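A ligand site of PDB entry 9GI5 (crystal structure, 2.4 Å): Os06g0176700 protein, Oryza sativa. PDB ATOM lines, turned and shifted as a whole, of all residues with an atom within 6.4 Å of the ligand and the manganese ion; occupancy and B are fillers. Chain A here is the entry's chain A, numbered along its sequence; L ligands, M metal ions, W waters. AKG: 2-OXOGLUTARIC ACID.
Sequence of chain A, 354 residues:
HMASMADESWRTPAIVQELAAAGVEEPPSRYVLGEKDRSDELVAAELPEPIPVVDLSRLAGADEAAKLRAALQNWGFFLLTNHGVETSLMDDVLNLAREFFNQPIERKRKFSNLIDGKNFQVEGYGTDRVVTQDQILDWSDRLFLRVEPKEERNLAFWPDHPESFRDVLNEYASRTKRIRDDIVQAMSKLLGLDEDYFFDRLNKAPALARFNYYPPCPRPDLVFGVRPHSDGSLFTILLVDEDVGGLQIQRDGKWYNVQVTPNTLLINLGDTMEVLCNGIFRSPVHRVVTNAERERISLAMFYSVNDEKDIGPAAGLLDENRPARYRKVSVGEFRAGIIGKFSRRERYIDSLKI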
ATOM      1  N   ARG A 210     -25.447  16.332  31.542  1.00  0.00           N
ATOM      2  CA  ARG A 210     -25.218  17.646  32.122  1.00  0.00           C
ATOM      3  C   ARG A 210     -26.572  18.267  32.449  1.00  0.00           C
ATOM      4  O   ARG A 210     -27.299  18.691  31.545  1.00  0.00           O
ATOM      5  CB  ARG A 210     -24.407  18.533  31.167  1.00  0.00           C
ATOM      6  CG  ARG A 210     -23.952  19.872  31.784  1.00  0.00           C
ATOM      7  CD  ARG A 210     -23.276  20.777  30.747  1.00  0.00           C
ATOM      8  NE  ARG A 210     -22.978  22.113  31.259  1.00  0.00           N
ATOM      9  CZ  ARG A 210     -21.776  22.535  31.620  1.00  0.00           C
ATOM     10  NH1 ARG A 210     -20.719  21.745  31.539  1.00  0.00           N
ATOM     11  NH2 ARG A 210     -21.628  23.775  32.075  1.00  0.00           N
ATOM     12  N   ASN A 212     -28.229  21.361  33.618  1.00  0.00           N
ATOM     13  CA  ASN A 212     -27.928  22.771  33.750  1.00  0.00           C
ATOM     14  C   ASN A 212     -28.975  23.465  34.594  1.00  0.00           C
ATOM     15  O   ASN A 212     -30.178  23.183  34.486  1.00  0.00           O
ATOM     16  CB  ASN A 212     -27.854  23.455  32.372  1.00  0.00           C
ATOM     17  CG  ASN A 212     -26.769  22.877  31.511  1.00  0.00           C
ATOM     18  OD1 ASN A 212     -25.580  22.990  31.818  1.00  0.00           O
ATOM     19  ND2 ASN A 212     -27.163  22.261  30.388  1.00  0.00           N
ATOM     20  N   TYR A 214     -29.914  27.395  35.245  1.00  0.00           N
ATOM     21  CA  TYR A 214     -29.663  28.799  34.997  1.00  0.00           C
ATOM     22  C   TYR A 214     -30.536  29.615  35.940  1.00  0.00           C
ATOM     23  O   TYR A 214     -31.754  29.734  35.704  1.00  0.00           O
ATOM     24  CB  TYR A 214     -29.957  29.162  33.541  1.00  0.00           C
ATOM     25  CG  TYR A 214     -29.338  28.243  32.503  1.00  0.00           C
ATOM     26  CD1 TYR A 214     -30.002  27.096  32.077  1.00  0.00           C
ATOM     27  CD2 TYR A 214     -28.104  28.529  31.945  1.00  0.00           C
ATOM     28  CE1 TYR A 214     -29.455  26.258  31.120  1.00  0.00           C
ATOM     29  CE2 TYR A 214     -27.537  27.686  30.976  1.00  0.00           C
ATOM     30  CZ  TYR A 214     -28.230  26.551  30.570  1.00  0.00           C
ATOM     31  OH  TYR A 214     -27.683  25.715  29.623  1.00  0.00           O
ATOM     32  N   VAL A 226     -24.857  30.333  29.701  1.00  0.00           N
ATOM     33  CA  VAL A 226     -23.667  29.610  29.278  1.00  0.00           C
ATOM     34  C   VAL A 226     -23.079  30.292  28.055  1.00  0.00           C
ATOM     35  O   VAL A 226     -23.804  30.743  27.164  1.00  0.00           O
ATOM     36  CB  VAL A 226     -23.933  28.108  29.010  1.00  0.00           C
ATOM     37  CG1 VAL A 226     -24.848  27.896  27.815  1.00  0.00           C
ATOM     38  CG2 VAL A 226     -22.618  27.356  28.853  1.00  0.00           C
ATOM     39  N   HIS A 229     -20.644  28.570  22.419  1.00  0.00           N
ATOM     40  CA  HIS A 229     -19.782  27.401  22.254  1.00  0.00           C
ATOM     41  C   HIS A 229     -20.457  26.445  21.290  1.00  0.00           C
ATOM     42  O   HIS A 229     -21.675  26.459  21.127  1.00  0.00           O
ATOM     43  CB  HIS A 229     -19.530  26.713  23.602  1.00  0.00           C
ATOM     44  CG  HIS A 229     -20.741  26.014  24.133  1.00  0.00           C
ATOM     45  ND1 HIS A 229     -21.775  26.678  24.753  1.00  0.00           N
ATOM     46  CD2 HIS A 229     -21.075  24.698  24.145  1.00  0.00           C
ATOM     47  CE1 HIS A 229     -22.701  25.801  25.110  1.00  0.00           C
ATOM     48  NE2 HIS A 229     -22.305  24.595  24.754  1.00  0.00           N
ATOM     49  N   SER A 230     -19.641  25.601  20.678  1.00  0.00           N
ATOM     50  CA  SER A 230     -20.149  24.376  20.065  1.00  0.00           C
ATOM     51  C   SER A 230     -19.830  23.212  20.988  1.00  0.00           C
ATOM     52  O   SER A 230     -18.875  23.266  21.774  1.00  0.00           O
ATOM     53  CB  SER A 230     -19.527  24.140  18.689  1.00  0.00           C
ATOM     54  OG  SER A 230     -18.110  24.138  18.749  1.00  0.00           O
ATOM     55  N   ASP A 231     -20.631  22.164  20.897  1.00  0.00           N
ATOM     56  CA  ASP A 231     -20.390  20.975  21.701  1.00  0.00           C
ATOM     57  C   ASP A 231     -19.199  20.203  21.145  1.00  0.00           C
ATOM     58  O   ASP A 231     -18.916  20.234  19.944  1.00  0.00           O
ATOM     59  CB  ASP A 231     -21.631  20.083  21.725  1.00  0.00           C
ATOM     60  CG  ASP A 231     -22.797  20.719  22.496  1.00  0.00           C
ATOM     61  OD1 ASP A 231     -22.546  21.673  23.264  1.00  0.00           O
ATOM     62  OD2 ASP A 231     -23.950  20.250  22.342  1.00  0.00           O
ATOM     63  N   THR A 236     -25.415  15.692  20.484  1.00  0.00           N
ATOM     64  CA  THR A 236     -25.965  16.104  21.768  1.00  0.00           C
ATOM     65  C   THR A 236     -27.478  15.989  21.702  1.00  0.00           C
ATOM     66  O   THR A 236     -28.093  16.406  20.713  1.00  0.00           O
ATOM     67  CB  THR A 236     -25.553  17.543  22.109  1.00  0.00           C
ATOM     68  OG1 THR A 236     -24.123  17.630  22.172  1.00  0.00           O
ATOM     69  CG2 THR A 236     -26.144  17.966  23.426  1.00  0.00           C
ATOM     70  N   LEU A 238     -30.731  17.161  23.823  1.00  0.00           N
ATOM     71  CA  LEU A 238     -31.045  18.167  24.827  1.00  0.00           C
ATOM     72  C   LEU A 238     -32.515  18.089  25.187  1.00  0.00           C
ATOM     73  O   LEU A 238     -33.375  17.997  24.305  1.00  0.00           O
ATOM     74  CB  LEU A 238     -30.700  19.566  24.306  1.00  0.00           C
ATOM     75  CG  LEU A 238     -31.068  20.766  25.176  1.00  0.00           C
ATOM     76  CD1 LEU A 238     -30.314  20.740  26.494  1.00  0.00           C
ATOM     77  CD2 LEU A 238     -30.793  22.061  24.432  1.00  0.00           C
ATOM     78  N   VAL A 240     -35.340  20.131  27.805  1.00  0.00           N
ATOM     79  CA  VAL A 240     -35.513  21.373  28.553  1.00  0.00           C
ATOM     80  C   VAL A 240     -36.842  21.345  29.289  1.00  0.00           C
ATOM     81  O   VAL A 240     -37.879  20.993  28.707  1.00  0.00           O
ATOM     82  CB  VAL A 240     -35.432  22.614  27.639  1.00  0.00           C
ATOM     83  CG1 VAL A 240     -35.381  23.882  28.487  1.00  0.00           C
ATOM     84  CG2 VAL A 240     -34.210  22.536  26.717  1.00  0.00           C
ATOM     85  N   ASP A 243     -39.316  25.220  28.409  1.00  0.00           N
ATOM     86  CA  ASP A 243     -38.177  26.048  27.997  1.00  0.00           C
ATOM     87  C   ASP A 243     -38.230  27.525  28.355  1.00  0.00           C
ATOM     88  O   ASP A 243     -37.174  28.136  28.564  1.00  0.00           O
ATOM     89  CB  ASP A 243     -37.973  25.914  26.487  1.00  0.00           C
ATOM     90  CG  ASP A 243     -36.529  26.135  26.088  1.00  0.00           C
ATOM     91  OD1 ASP A 243     -35.916  27.100  26.596  1.00  0.00           O
ATOM     92  OD2 ASP A 243     -36.008  25.342  25.289  1.00  0.00           O
ATOM     93  N   GLY A 246     -34.348  31.224  26.099  1.00  0.00           N
ATOM     94  CA  GLY A 246     -32.974  31.478  26.478  1.00  0.00           C
ATOM     95  C   GLY A 246     -31.936  30.851  25.573  1.00  0.00           C
ATOM     96  O   GLY A 246     -30.836  31.400  25.416  1.00  0.00           O
ATOM     97  N   LEU A 247     -32.245  29.707  24.985  1.00  0.00           N
ATOM     98  CA  LEU A 247     -31.295  29.085  24.069  1.00  0.00           C
ATOM     99  C   LEU A 247     -31.228  29.889  22.783  1.00  0.00           C
ATOM    100  O   LEU A 247     -32.255  30.183  22.166  1.00  0.00           O
ATOM    101  CB  LEU A 247     -31.688  27.640  23.770  1.00  0.00           C
ATOM    102  CG  LEU A 247     -30.773  26.923  22.771  1.00  0.00           C
ATOM    103  CD1 LEU A 247     -29.325  26.957  23.236  1.00  0.00           C
ATOM    104  CD2 LEU A 247     -31.230  25.489  22.508  1.00  0.00           C
ATOM    105  N   VAL A 260     -37.020  24.992  22.854  1.00  0.00           N
ATOM    106  CA  VAL A 260     -37.164  23.539  22.766  1.00  0.00           C
ATOM    107  C   VAL A 260     -38.522  23.168  23.366  1.00  0.00           C
ATOM    108  O   VAL A 260     -38.684  23.173  24.583  1.00  0.00           O
ATOM    109  CB  VAL A 260     -36.028  22.809  23.487  1.00  0.00           C
ATOM    110  CG1 VAL A 260     -36.102  21.308  23.205  1.00  0.00           C
ATOM    111  CG2 VAL A 260     -34.686  23.378  23.083  1.00  0.00           C
ATOM    112  N   ASN A 268     -28.326  18.337  18.301  1.00  0.00           N
ATOM    113  CA  ASN A 268     -27.377  19.129  17.546  1.00  0.00           C
ATOM    114  C   ASN A 268     -26.113  18.319  17.286  1.00  0.00           C
ATOM    115  O   ASN A 268     -25.740  17.446  18.074  1.00  0.00           O
ATOM    116  CB  ASN A 268     -27.036  20.448  18.236  1.00  0.00           C
ATOM    117  CG  ASN A 268     -26.379  20.236  19.559  1.00  0.00           C
ATOM    118  OD1 ASN A 268     -27.034  19.867  20.530  1.00  0.00           O
ATOM    119  ND2 ASN A 268     -25.070  20.479  19.613  1.00  0.00           N
ATOM    120  N   HIS A 286     -23.784  27.896  19.955  1.00  0.00           N
ATOM    121  CA  HIS A 286     -25.023  28.214  20.629  1.00  0.00           C
ATOM    122  C   HIS A 286     -24.709  28.754  22.016  1.00  0.00           C
ATOM    123  O   HIS A 286     -23.578  28.632  22.505  1.00  0.00           O
ATOM    124  CB  HIS A 286     -25.942  26.991  20.700  1.00  0.00           C
ATOM    125  CG  HIS A 286     -25.293  25.771  21.261  1.00  0.00           C
ATOM    126  ND1 HIS A 286     -24.346  25.045  20.576  1.00  0.00           N
ATOM    127  CD2 HIS A 286     -25.438  25.158  22.469  1.00  0.00           C
ATOM    128  CE1 HIS A 286     -23.948  24.024  21.320  1.00  0.00           C
ATOM    129  NE2 HIS A 286     -24.593  24.074  22.481  1.00  0.00           N
ATOM    130  N   ARG A 287     -25.712  29.349  22.652  1.00  0.00           N
ATOM    131  CA  ARG A 287     -25.523  29.970  23.947  1.00  0.00           C
ATOM    132  C   ARG A 287     -26.874  30.050  24.654  1.00  0.00           C
ATOM    133  O   ARG A 287     -27.930  29.875  24.043  1.00  0.00           O
ATOM    134  CB  ARG A 287     -24.897  31.364  23.822  1.00  0.00           C
ATOM    135  CG  ARG A 287     -25.884  32.438  23.411  1.00  0.00           C
ATOM    136  CD  ARG A 287     -25.197  33.694  22.930  1.00  0.00           C
ATOM    137  NE  ARG A 287     -26.175  34.677  22.481  1.00  0.00           N
ATOM    138  CZ  ARG A 287     -25.865  35.855  21.957  1.00  0.00           C
ATOM    139  NH1 ARG A 287     -24.600  36.222  21.801  1.00  0.00           N
ATOM    140  NH2 ARG A 287     -26.837  36.681  21.606  1.00  0.00           N
ATOM    141  N   VAL A 288     -26.823  30.340  25.949  1.00  0.00           N
ATOM    142  CA  VAL A 288     -28.018  30.552  26.754  1.00  0.00           C
ATOM    143  C   VAL A 288     -27.926  31.911  27.423  1.00  0.00           C
ATOM    144  O   VAL A 288     -26.945  32.205  28.124  1.00  0.00           O
ATOM    145  CB  VAL A 288     -28.215  29.441  27.791  1.00  0.00           C
ATOM    146  CG1 VAL A 288     -29.413  29.760  28.692  1.00  0.00           C
ATOM    147  CG2 VAL A 288     -28.413  28.094  27.101  1.00  0.00           C
ATOM    148  N   ARG A 296     -34.102  28.311  34.683  1.00  0.00           N
ATOM    149  CA  ARG A 296     -34.283  27.452  33.531  1.00  0.00           C
ATOM    150  C   ARG A 296     -33.471  26.184  33.770  1.00  0.00           C
ATOM    151  O   ARG A 296     -32.311  26.267  34.185  1.00  0.00           O
ATOM    152  CB  ARG A 296     -33.841  28.154  32.248  1.00  0.00           C
ATOM    153  CG  ARG A 296     -33.957  27.349  30.977  1.00  0.00           C
ATOM    154  CD  ARG A 296     -33.642  28.223  29.754  1.00  0.00           C
ATOM    155  NE  ARG A 296     -33.794  27.479  28.501  1.00  0.00           N
ATOM    156  CZ  ARG A 296     -32.873  26.669  28.002  1.00  0.00           C
ATOM    157  NH1 ARG A 296     -31.713  26.479  28.613  1.00  0.00           N
ATOM    158  NH2 ARG A 296     -33.133  26.005  26.877  1.00  0.00           N
ATOM    159  N   ILE A 297     -34.083  25.036  33.516  1.00  0.00           N
ATOM    160  CA  ILE A 297     -33.454  23.741  33.744  1.00  0.00           C
ATOM    161  C   ILE A 297     -33.420  22.984  32.430  1.00  0.00           C
ATOM    162  O   ILE A 297     -34.423  22.929  31.703  1.00  0.00           O
ATOM    163  CB  ILE A 297     -34.217  22.931  34.818  1.00  0.00           C
ATOM    164  CG1 ILE A 297     -34.009  23.551  36.205  1.00  0.00           C
ATOM    165  CG2 ILE A 297     -33.776  21.480  34.801  1.00  0.00           C
ATOM    166  CD1 ILE A 297     -34.621  22.730  37.335  1.00  0.00           C
ATOM    167  N   SER A 298     -32.257  22.409  32.114  1.00  0.00           N
ATOM    168  CA  SER A 298     -32.142  21.554  30.944  1.00  0.00           C
ATOM    169  C   SER A 298     -31.245  20.368  31.274  1.00  0.00           C
ATOM    170  O   SER A 298     -30.448  20.407  32.210  1.00  0.00           O
ATOM    171  CB  SER A 298     -31.594  22.335  29.739  1.00  0.00           C
ATOM    172  OG  SER A 298     -30.207  22.582  29.886  1.00  0.00           O
ATOM    173  N   LEU A 299     -31.407  19.304  30.495  1.00  0.00           N
ATOM    174  CA  LEU A 299     -30.517  18.156  30.562  1.00  0.00           C
ATOM    175  C   LEU A 299     -29.946  17.909  29.175  1.00  0.00           C
ATOM    176  O   LEU A 299     -30.691  17.794  28.202  1.00  0.00           O
ATOM    177  CB  LEU A 299     -31.244  16.910  31.077  1.00  0.00           C
ATOM    178  CG  LEU A 299     -30.507  15.583  30.818  1.00  0.00           C
ATOM    179  CD1 LEU A 299     -29.147  15.588  31.503  1.00  0.00           C
ATOM    180  CD2 LEU A 299     -31.342  14.389  31.289  1.00  0.00           C
ATOM    181  N   ALA A 300     -28.620  17.831  29.091  1.00  0.00           N
ATOM    182  CA  ALA A 300     -27.932  17.577  27.827  1.00  0.00           C
ATOM    183  C   ALA A 300     -27.139  16.288  27.948  1.00  0.00           C
ATOM    184  O   ALA A 300     -26.283  16.157  28.833  1.00  0.00           O
ATOM    185  CB  ALA A 300     -27.014  18.741  27.459  1.00  0.00           C
ATOM    186  N   PHE A 302     -24.370  14.268  26.224  1.00  0.00           N
ATOM    187  CA  PHE A 302     -23.299  14.330  25.238  1.00  0.00           C
ATOM    188  C   PHE A 302     -22.804  12.925  24.938  1.00  0.00           C
ATOM    189  O   PHE A 302     -22.485  12.150  25.851  1.00  0.00           O
ATOM    190  CB  PHE A 302     -22.132  15.189  25.737  1.00  0.00           C
ATOM    191  CG  PHE A 302     -22.534  16.583  26.175  1.00  0.00           C
ATOM    192  CD1 PHE A 302     -22.969  17.525  25.259  1.00  0.00           C
ATOM    193  CD2 PHE A 302     -22.457  16.948  27.518  1.00  0.00           C
ATOM    194  CE1 PHE A 302     -23.329  18.805  25.673  1.00  0.00           C
ATOM    195  CE2 PHE A 302     -22.817  18.227  27.932  1.00  0.00           C
ATOM    196  CZ  PHE A 302     -23.250  19.151  27.000  1.00  0.00           C
HETATM  197  C1  AKG L   1     -25.031  22.411  27.137  1.00  0.00           C
HETATM  198  O1  AKG L   1     -25.299  21.882  28.201  1.00  0.00           O
HETATM  199  O2  AKG L   1     -23.894  22.270  26.507  1.00  0.00           O
HETATM  200  C2  AKG L   1     -26.046  23.332  26.429  1.00  0.00           C
HETATM  201  O5  AKG L   1     -25.713  23.923  25.402  1.00  0.00           O
HETATM  202  C3  AKG L   1     -27.427  23.457  27.021  1.00  0.00           C
HETATM  203  C4  AKG L   1     -28.293  24.468  26.288  1.00  0.00           C
HETATM  204  C5  AKG L   1     -29.647  24.711  26.915  1.00  0.00           C
HETATM  205  O3  AKG L   1     -30.650  24.897  26.264  1.00  0.00           O
HETATM  206  O4  AKG L   1     -29.632  24.716  28.225  1.00  0.00           O
HETATM  207 MN    MN M   1     -23.868  22.977  24.372  1.00  0.00          MN
HETATM  208  O   HOH W   1     -26.057  21.488  23.729  1.00  0.00           O
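The backbone carbonyl oxygen (O) of Arg 296 sits at hydrogen-bond distance from the backbone NH (N) of Tyr 214.
The guanidinium group of Arg 210 lies within hydrogen-bond range of the side-chain amide oxygen of Asn 212 (2.8 Å).
OD2 of Asp 231 sits at hydrogen-bond distance from OG1 of Thr 236, at 2.6 Å.
NE of Arg 296 lies within salt-bridge range of OD1 of Asp 243 (2.9 Å).
The backbone carbonyl oxygen (O) of Val 288 lies within hydrogen-bond range of the backbone NH (N) of Val 226 (3.2 Å).
The side-chain carboxylate (OD2) of Asp 231 lies within hydrogen-bond range of the side-chain amide nitrogen (ND2) of Asn 268 (3.0 Å).
The backbone NH of Arg 210 is in hydrogen-bond range of the backbone carbonyl oxygen of Ala 300, at 2.8 Å.
The backbone NH of Asn 212 sits at hydrogen-bond distance from the backbone carbonyl oxygen of Ser 298 (2.8 Å).
The side-chain hydroxyl (OH) of Tyr 214 sits at hydrogen-bond distance from an oxygen (O4) of the ligand (2.6 Å).
The guanidinium group (NE) of Arg 210 is in salt-bridge range of an oxygen (O1) of the ligand, at 3.8 Å.
ND2 of Asn 212 is in hydrogen-bond range of O1 of the ligand (2.9 Å).
The guanidinium group of Arg 296 lies within salt-bridge range of an oxygen (O4) of the ligand, 2.8 Å away.
The side-chain hydroxyl (OG) of Ser 298 sits at hydrogen-bond distance from an oxygen (O4) of the ligand, 2.8 Å away.
Merely in contact with the ligand: Phe 302, Leu 238, Val 288, Ala 300 and Leu 247.
Hydrophobic or aromatic side chains that line the ligand: Tyr 214, His 229, Leu 238, Leu 247, His 286, Val 288, Ala 300 and Phe 302.
Within 4 Å of the ligand: Arg 210, Asn 212, Tyr 214, His 229, Asp 231, Leu 238, Leu 247, His 286, Val 288, Arg 296, Ser 298, Ala 300 and Phe 302.
The manganese ion is bound by the side-chain carboxylate (OD1) of Asp 231 (2.2 Å).
An oxygen (O2) of the ligand is bound to the manganese ion, at 2.2 Å.
NE2 of His 229 binds the manganese ion, at 2.3 Å.
The manganese ion is bound by a ring nitrogen (NE2) of His 286, at 2.3 Å.
An oxygen (O5) of the ligand binds the manganese ion (2.3 Å).
Slightly farther from the manganese ion lies water W1 (2.7 Å).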
